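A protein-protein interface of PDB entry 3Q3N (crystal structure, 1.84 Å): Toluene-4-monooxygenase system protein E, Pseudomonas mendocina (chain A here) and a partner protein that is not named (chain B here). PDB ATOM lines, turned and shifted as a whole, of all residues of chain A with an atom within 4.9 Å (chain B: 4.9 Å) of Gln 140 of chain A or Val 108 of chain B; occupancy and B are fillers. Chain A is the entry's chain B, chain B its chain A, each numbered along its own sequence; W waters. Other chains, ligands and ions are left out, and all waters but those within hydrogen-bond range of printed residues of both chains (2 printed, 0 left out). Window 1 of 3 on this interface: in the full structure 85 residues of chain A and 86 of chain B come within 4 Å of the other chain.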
ATOM      1  N   HIS A  33      -0.717   0.980  13.950  1.00  0.00           N
ATOM      2  CA  HIS A  33       0.167   0.856  12.779  1.00  0.00           C
ATOM      3  C   HIS A  33      -0.468  -0.070  11.749  1.00  0.00           C
ATOM      4  O   HIS A  33      -0.318  -1.281  11.850  1.00  0.00           O
ATOM      5  CB  HIS A  33       1.508   0.232  13.157  1.00  0.00           C
ATOM      6  CG  HIS A  33       2.454   1.151  13.861  1.00  0.00           C
ATOM      7  ND1 HIS A  33       2.378   2.525  13.772  1.00  0.00           N
ATOM      8  CD2 HIS A  33       3.519   0.881  14.651  1.00  0.00           C
ATOM      9  CE1 HIS A  33       3.361   3.063  14.475  1.00  0.00           C
ATOM     10  NE2 HIS A  33       4.061   2.085  15.027  1.00  0.00           N
ATOM     11  N   SER A 136      15.863   8.072  19.395  1.00  0.00           N
ATOM     12  CA  SER A 136      14.536   7.736  19.887  1.00  0.00           C
ATOM     13  C   SER A 136      13.491   7.877  18.789  1.00  0.00           C
ATOM     14  O   SER A 136      12.580   7.050  18.680  1.00  0.00           O
ATOM     15  CB  SER A 136      14.170   8.613  21.086  1.00  0.00           C
ATOM     16  OG  SER A 136      15.030   8.314  22.176  1.00  0.00           O
ATOM     17  N   ALA A 137      13.625   8.929  17.979  1.00  0.00           N
ATOM     18  CA  ALA A 137      12.688   9.156  16.889  1.00  0.00           C
ATOM     19  C   ALA A 137      12.799   8.028  15.877  1.00  0.00           C
ATOM     20  O   ALA A 137      11.809   7.642  15.256  1.00  0.00           O
ATOM     21  CB  ALA A 137      12.946  10.520  16.201  1.00  0.00           C
ATOM     22  N   TYR A 138      14.007   7.507  15.677  1.00  0.00           N
ATOM     23  CA  TYR A 138      14.133   6.401  14.735  1.00  0.00           C
ATOM     24  C   TYR A 138      13.416   5.132  15.233  1.00  0.00           C
ATOM     25  O   TYR A 138      12.718   4.449  14.471  1.00  0.00           O
ATOM     26  CB  TYR A 138      15.596   6.088  14.395  1.00  0.00           C
ATOM     27  CG  TYR A 138      15.687   5.029  13.321  1.00  0.00           C
ATOM     28  CD1 TYR A 138      16.123   3.735  13.616  1.00  0.00           C
ATOM     29  CD2 TYR A 138      15.296   5.311  12.017  1.00  0.00           C
ATOM     30  CE1 TYR A 138      16.184   2.762  12.621  1.00  0.00           C
ATOM     31  CE2 TYR A 138      15.351   4.344  11.021  1.00  0.00           C
ATOM     32  CZ  TYR A 138      15.791   3.073  11.330  1.00  0.00           C
ATOM     33  OH  TYR A 138      15.842   2.108  10.339  1.00  0.00           O
ATOM     34  N   VAL A 139      13.595   4.795  16.503  1.00  0.00           N
ATOM     35  CA  VAL A 139      12.886   3.629  17.019  1.00  0.00           C
ATOM     36  C   VAL A 139      11.376   3.859  16.890  1.00  0.00           C
ATOM     37  O   VAL A 139      10.638   2.946  16.515  1.00  0.00           O
ATOM     38  CB  VAL A 139      13.292   3.260  18.462  1.00  0.00           C
ATOM     39  CG1 VAL A 139      12.603   1.950  18.881  1.00  0.00           C
ATOM     40  CG2 VAL A 139      14.808   3.086  18.552  1.00  0.00           C
ATOM     41  N   GLN A 140      10.925   5.088  17.154  1.00  0.00           N
ATOM     42  CA  GLN A 140       9.516   5.432  16.961  1.00  0.00           C
ATOM     43  C   GLN A 140       9.020   5.014  15.577  1.00  0.00           C
ATOM     44  O   GLN A 140       8.018   4.311  15.446  1.00  0.00           O
ATOM     45  CB  GLN A 140       9.283   6.944  17.156  1.00  0.00           C
ATOM     46  CG  GLN A 140       7.872   7.441  16.768  1.00  0.00           C
ATOM     47  CD  GLN A 140       7.694   7.689  15.262  1.00  0.00           C
ATOM     48  OE1 GLN A 140       8.521   8.350  14.617  1.00  0.00           O
ATOM     49  NE2 GLN A 140       6.610   7.153  14.699  1.00  0.00           N
ATOM     50  N   GLN A 141       9.709   5.461  14.534  1.00  0.00           N
ATOM     51  CA  GLN A 141       9.166   5.291  13.188  1.00  0.00           C
ATOM     52  C   GLN A 141       9.264   3.849  12.675  1.00  0.00           C
ATOM     53  O   GLN A 141       8.540   3.459  11.757  1.00  0.00           O
ATOM     54  CB  GLN A 141       9.812   6.286  12.208  1.00  0.00           C
ATOM     55  CG  GLN A 141      11.298   6.072  11.970  1.00  0.00           C
ATOM     56  CD  GLN A 141      11.988   7.378  11.555  1.00  0.00           C
ATOM     57  OE1 GLN A 141      12.193   8.266  12.387  1.00  0.00           O
ATOM     58  NE2 GLN A 141      12.336   7.498  10.272  1.00  0.00           N
ATOM     59  N   MET A 142      10.129   3.055  13.300  1.00  0.00           N
ATOM     60  CA  MET A 142      10.375   1.685  12.851  1.00  0.00           C
ATOM     61  C   MET A 142       9.690   0.594  13.695  1.00  0.00           C
ATOM     62  O   MET A 142       9.532  -0.536  13.236  1.00  0.00           O
ATOM     63  CB  MET A 142      11.881   1.392  12.808  1.00  0.00           C
ATOM     64  CG  MET A 142      12.681   2.235  11.821  1.00  0.00           C
ATOM     65  SD  MET A 142      11.976   2.353  10.157  1.00  0.00           S
ATOM     66  CE  MET A 142      11.841   0.653   9.660  1.00  0.00           C
ATOM     67  N   ALA A 143       9.293   0.915  14.921  1.00  0.00           N
ATOM     68  CA  ALA A 143       8.755  -0.124  15.814  1.00  0.00           C
ATOM     69  C   ALA A 143       7.476  -0.758  15.255  1.00  0.00           C
ATOM     70  O   ALA A 143       6.664  -0.079  14.635  1.00  0.00           O
ATOM     71  CB  ALA A 143       8.495   0.450  17.222  1.00  0.00           C
ATOM     72  N   SER A 149       5.807   2.426  19.769  1.00  0.00           N
ATOM     73  CA  SER A 149       6.167   3.723  19.191  1.00  0.00           C
ATOM     74  C   SER A 149       5.795   4.882  20.120  1.00  0.00           C
ATOM     75  O   SER A 149       6.540   5.855  20.236  1.00  0.00           O
ATOM     76  CB  SER A 149       5.515   3.914  17.826  1.00  0.00           C
ATOM     77  OG  SER A 149       6.064   2.975  16.910  1.00  0.00           O
ATOM     78  N   CYS A 152       8.312   5.583  22.546  1.00  0.00           N
ATOM     79  CA  CYS A 152       9.437   6.228  21.882  1.00  0.00           C
ATOM     80  C   CYS A 152       9.174   7.708  21.610  1.00  0.00           C
ATOM     81  O   CYS A 152      10.097   8.517  21.644  1.00  0.00           O
ATOM     82  CB  CYS A 152       9.778   5.515  20.565  1.00  0.00           C
ATOM     83  SG  CYS A 152      10.356   3.827  20.779  1.00  0.00           S
ATOM     84  N   ILE A 153       7.934   8.058  21.303  1.00  0.00           N
ATOM     85  CA  ILE A 153       7.616   9.467  21.072  1.00  0.00           C
ATOM     86  C   ILE A 153       7.882  10.261  22.342  1.00  0.00           C
ATOM     87  O   ILE A 153       8.543  11.304  22.328  1.00  0.00           O
ATOM     88  CB  ILE A 153       6.145   9.675  20.648  1.00  0.00           C
ATOM     89  CG1 ILE A 153       5.855   8.953  19.327  1.00  0.00           C
ATOM     90  CG2 ILE A 153       5.807  11.197  20.538  1.00  0.00           C
ATOM     91  CD1 ILE A 153       4.366   8.800  19.046  1.00  0.00           C
ATOM     92  N   GLU B 104      -3.728  10.895  11.189  1.00  0.00           N
ATOM     93  CA  GLU B 104      -3.036  11.786  12.122  1.00  0.00           C
ATOM     94  C   GLU B 104      -1.932  10.995  12.807  1.00  0.00           C
ATOM     95  O   GLU B 104      -0.815  11.480  12.969  1.00  0.00           O
ATOM     96  CB  GLU B 104      -3.997  12.332  13.193  1.00  0.00           C
ATOM     97  CG  GLU B 104      -5.113  13.210  12.656  1.00  0.00           C
ATOM     98  CD  GLU B 104      -4.770  14.681  12.712  1.00  0.00           C
ATOM     99  OE1 GLU B 104      -5.693  15.524  12.744  1.00  0.00           O
ATOM    100  OE2 GLU B 104      -3.571  14.995  12.717  1.00  0.00           O
ATOM    101  N   TYR B 105      -2.243   9.772  13.230  1.00  0.00           N
ATOM    102  CA  TYR B 105      -1.236   8.985  13.937  1.00  0.00           C
ATOM    103  C   TYR B 105      -0.093   8.616  12.974  1.00  0.00           C
ATOM    104  O   TYR B 105       1.084   8.600  13.356  1.00  0.00           O
ATOM    105  CB  TYR B 105      -1.839   7.732  14.611  1.00  0.00           C
ATOM    106  CG  TYR B 105      -0.805   7.009  15.450  1.00  0.00           C
ATOM    107  CD1 TYR B 105      -0.413   7.514  16.689  1.00  0.00           C
ATOM    108  CD2 TYR B 105      -0.178   5.858  14.983  1.00  0.00           C
ATOM    109  CE1 TYR B 105       0.550   6.860  17.458  1.00  0.00           C
ATOM    110  CE2 TYR B 105       0.787   5.208  15.740  1.00  0.00           C
ATOM    111  CZ  TYR B 105       1.145   5.717  16.968  1.00  0.00           C
ATOM    112  OH  TYR B 105       2.114   5.084  17.704  1.00  0.00           O
ATOM    113  N   ALA B 106      -0.439   8.320  11.725  1.00  0.00           N
ATOM    114  CA  ALA B 106       0.578   8.116  10.694  1.00  0.00           C
ATOM    115  C   ALA B 106       1.462   9.363  10.527  1.00  0.00           C
ATOM    116  O   ALA B 106       2.657   9.254  10.275  1.00  0.00           O
ATOM    117  CB  ALA B 106      -0.072   7.718   9.342  1.00  0.00           C
ATOM    118  N   ALA B 107       0.886  10.551  10.671  1.00  0.00           N
ATOM    119  CA  ALA B 107       1.692  11.776  10.554  1.00  0.00           C
ATOM    120  C   ALA B 107       2.802  11.885  11.607  1.00  0.00           C
ATOM    121  O   ALA B 107       3.788  12.589  11.397  1.00  0.00           O
ATOM    122  CB  ALA B 107       0.803  13.013  10.580  1.00  0.00           C
ATOM    123  N   VAL B 108       2.660  11.186  12.736  1.00  0.00           N
ATOM    124  CA  VAL B 108       3.746  11.134  13.710  1.00  0.00           C
ATOM    125  C   VAL B 108       5.025  10.629  13.021  1.00  0.00           C
ATOM    126  O   VAL B 108       6.135  11.125  13.278  1.00  0.00           O
ATOM    127  CB  VAL B 108       3.436  10.179  14.887  1.00  0.00           C
ATOM    128  CG1 VAL B 108       4.679  10.007  15.753  1.00  0.00           C
ATOM    129  CG2 VAL B 108       2.233  10.676  15.725  1.00  0.00           C
ATOM    130  N   THR B 109       4.853   9.661  12.125  1.00  0.00           N
ATOM    131  CA  THR B 109       5.982   9.048  11.404  1.00  0.00           C
ATOM    132  C   THR B 109       6.653  10.003  10.398  1.00  0.00           C
ATOM    133  O   THR B 109       7.873  10.022  10.268  1.00  0.00           O
ATOM    134  CB  THR B 109       5.568   7.722  10.723  1.00  0.00           C
ATOM    135  OG1 THR B 109       5.329   6.721  11.734  1.00  0.00           O
ATOM    136  CG2 THR B 109       6.674   7.217   9.773  1.00  0.00           C
ATOM    137  N   GLY B 110       5.856  10.796   9.694  1.00  0.00           N
ATOM    138  CA  GLY B 110       6.410  11.863   8.875  1.00  0.00           C
ATOM    139  C   GLY B 110       7.253  12.824   9.707  1.00  0.00           C
ATOM    140  O   GLY B 110       8.353  13.213   9.303  1.00  0.00           O
ATOM    141  N   GLU B 111       6.738  13.242  10.856  1.00  0.00           N
ATOM    142  CA  GLU B 111       7.502  14.136  11.726  1.00  0.00           C
ATOM    143  C   GLU B 111       8.750  13.398  12.238  1.00  0.00           C
ATOM    144  O   GLU B 111       9.840  13.953  12.284  1.00  0.00           O
ATOM    145  CB  GLU B 111       6.623  14.624  12.886  1.00  0.00           C
ATOM    146  CG  GLU B 111       5.462  15.543  12.415  1.00  0.00           C
ATOM    147  CD  GLU B 111       5.917  16.953  12.058  1.00  0.00           C
ATOM    148  OE1 GLU B 111       7.073  17.285  12.359  1.00  0.00           O
ATOM    149  OE2 GLU B 111       5.126  17.736  11.475  1.00  0.00           O
ATOM    150  N   GLY B 112       8.592  12.133  12.598  1.00  0.00           N
ATOM    151  CA  GLY B 112       9.722  11.346  13.069  1.00  0.00           C
ATOM    152  C   GLY B 112      10.828  11.208  12.029  1.00  0.00           C
ATOM    153  O   GLY B 112      12.019  11.179  12.355  1.00  0.00           O
ATOM    154  N   MET B 131       5.945  15.503  16.216  1.00  0.00           N
ATOM    155  CA  MET B 131       5.605  14.127  16.580  1.00  0.00           C
ATOM    156  C   MET B 131       4.587  14.154  17.711  1.00  0.00           C
ATOM    157  O   MET B 131       3.605  13.413  17.719  1.00  0.00           O
ATOM    158  CB  MET B 131       6.850  13.368  17.064  1.00  0.00           C
ATOM    159  CG  MET B 131       7.901  13.109  15.971  1.00  0.00           C
ATOM    160  SD  MET B 131       9.488  12.571  16.645  1.00  0.00           S
ATOM    161  CE  MET B 131       9.072  10.945  17.317  1.00  0.00           C
ATOM    162  N   GLU B 134       1.031  15.387  16.498  1.00  0.00           N
ATOM    163  CA  GLU B 134       0.217  14.419  15.760  1.00  0.00           C
ATOM    164  C   GLU B 134      -0.244  13.277  16.660  1.00  0.00           C
ATOM    165  O   GLU B 134      -1.309  12.711  16.457  1.00  0.00           O
ATOM    166  CB  GLU B 134       0.955  13.876  14.538  1.00  0.00           C
ATOM    167  CG  GLU B 134       1.441  14.947  13.554  1.00  0.00           C
ATOM    168  CD  GLU B 134       0.320  15.784  12.927  1.00  0.00           C
ATOM    169  OE1 GLU B 134      -0.878  15.668  13.307  1.00  0.00           O
ATOM    170  OE2 GLU B 134       0.655  16.588  12.033  1.00  0.00           O
ATOM    171  N   LEU B 135       0.564  12.936  17.656  1.00  0.00           N
ATOM    172  CA  LEU B 135       0.125  11.984  18.669  1.00  0.00           C
ATOM    173  C   LEU B 135      -1.149  12.511  19.347  1.00  0.00           C
ATOM    174  O   LEU B 135      -2.143  11.792  19.480  1.00  0.00           O
ATOM    175  CB  LEU B 135       1.232  11.749  19.695  1.00  0.00           C
ATOM    176  CG  LEU B 135       0.861  10.743  20.795  1.00  0.00           C
ATOM    177  CD1 LEU B 135       0.605   9.361  20.204  1.00  0.00           C
ATOM    178  CD2 LEU B 135       1.951  10.699  21.847  1.00  0.00           C
HETATM  179  O   HOH W   1       5.962   4.231  11.073  1.00  0.00           O
HETATM  180  O   HOH W   2       4.148   6.140  15.738  1.00  0.00           O
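Water W1 bridges the side-chain hydroxyl (OG1) of Thr 109 of chain B and the backbone carbonyl oxygen (O) of Gln 141 of chain A. Water W2 lies within hydrogen-bond range of the side-chain amide nitrogen (NE2) of Gln 140 of chain A (2.9 Å) and the side-chain hydroxyl (OH) of Tyr 105 of chain B (3.0 Å).
The side-chain hydroxyl of Thr 109 of chain B lies within hydrogen-bond range of the side-chain amide nitrogen of Gln 140 of chain A, 3.3 Å away. The backbone carbonyl oxygen (O) of Gly 112 of chain B sits close to the side-chain amide oxygen (OE1) of Gln 141 of chain A (2.9 Å).
Tyr 105 of chain B touches His 33 of chain A. CG1 of Val 108 of chain B touches NE2 of Gln 140 of chain A (3.6 Å). CA of Gly 112 of chain B touches OE1 of Gln 140 of chain A (3.6 Å). Gln 140 of chain A touches Met 131 of chain B (CG to CE, 3.7 Å). CB of Ser 149 of chain A touches OH of Tyr 105 of chain B (3.6 Å). Ile 153 of chain A touches Val 108 of chain B. Ile 153 of chain A touches Leu 135 of chain B.
Gln 140 of chain A touches just these residues of chain B: Val 108 (3.6 Å), Thr 109 (3.3 Å), Gly 112 (3.6 Å) and Met 131 (3.7 Å). Val 108 of chain B touches just these residues of chain A: Gln 140 (3.6 Å) and Ile 153 (3.5 Å). Of the printed residues of chain B, Ile 153 of chain A touches Val 108 and Leu 135. Of the printed residues of chain A, Leu 135 of chain B touches Ile 153 (3.98 Å). Of the printed residues of chain B, His 33 of chain A touches Tyr 105. The nearest printed residue of chain B that does not touch Ile 153 of chain A is Met 131 of chain B (4.2 Å).
O of Ala 137 of chain A sits close to OE1 of Gln 141 of chain A (3.0 Å). A ring nitrogen (NE2) of His 33 of chain A lies within hydrogen-bond range of the side-chain hydroxyl (OG) of Ser 149 of chain A (2.9 Å). O of Ala 137 of chain A sits close to OE1 of Gln 140 of chain A (3.4 Å). The backbone carbonyl oxygen (O) of Ala 143 of chain A sits close to a ring nitrogen (NE2) of His 33 of chain A, at 3.4 Å. The side-chain hydroxyl (OG) of Ser 149 of chain A lies within hydrogen-bond range of the backbone carbonyl oxygen (O) of Gln 140 of chain A (2.8 Å).
Hydrophobic or aromatic side chains of chain A that line the printed part of chain B: His 33 and Ile 153. Of the 12 printed residues of chain B, 6 touch a printed residue of chain A. Printed residues of chain B that touch a printed residue of chain A: Tyr 105, Val 108, Thr 109, Gly 112, Met 131 and Leu 135. Hydrophobic or aromatic side chains of chain B within 4 Å of the printed part of chain A: Tyr 105, Val 108, Met 131 and Leu 135. Among the printed residues, 9 pairs touch across the chains. Among the printed residues, no Asp or Glu carboxylate lies within 4 Å of a Lys or Arg side-chain nitrogen of the other chain.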
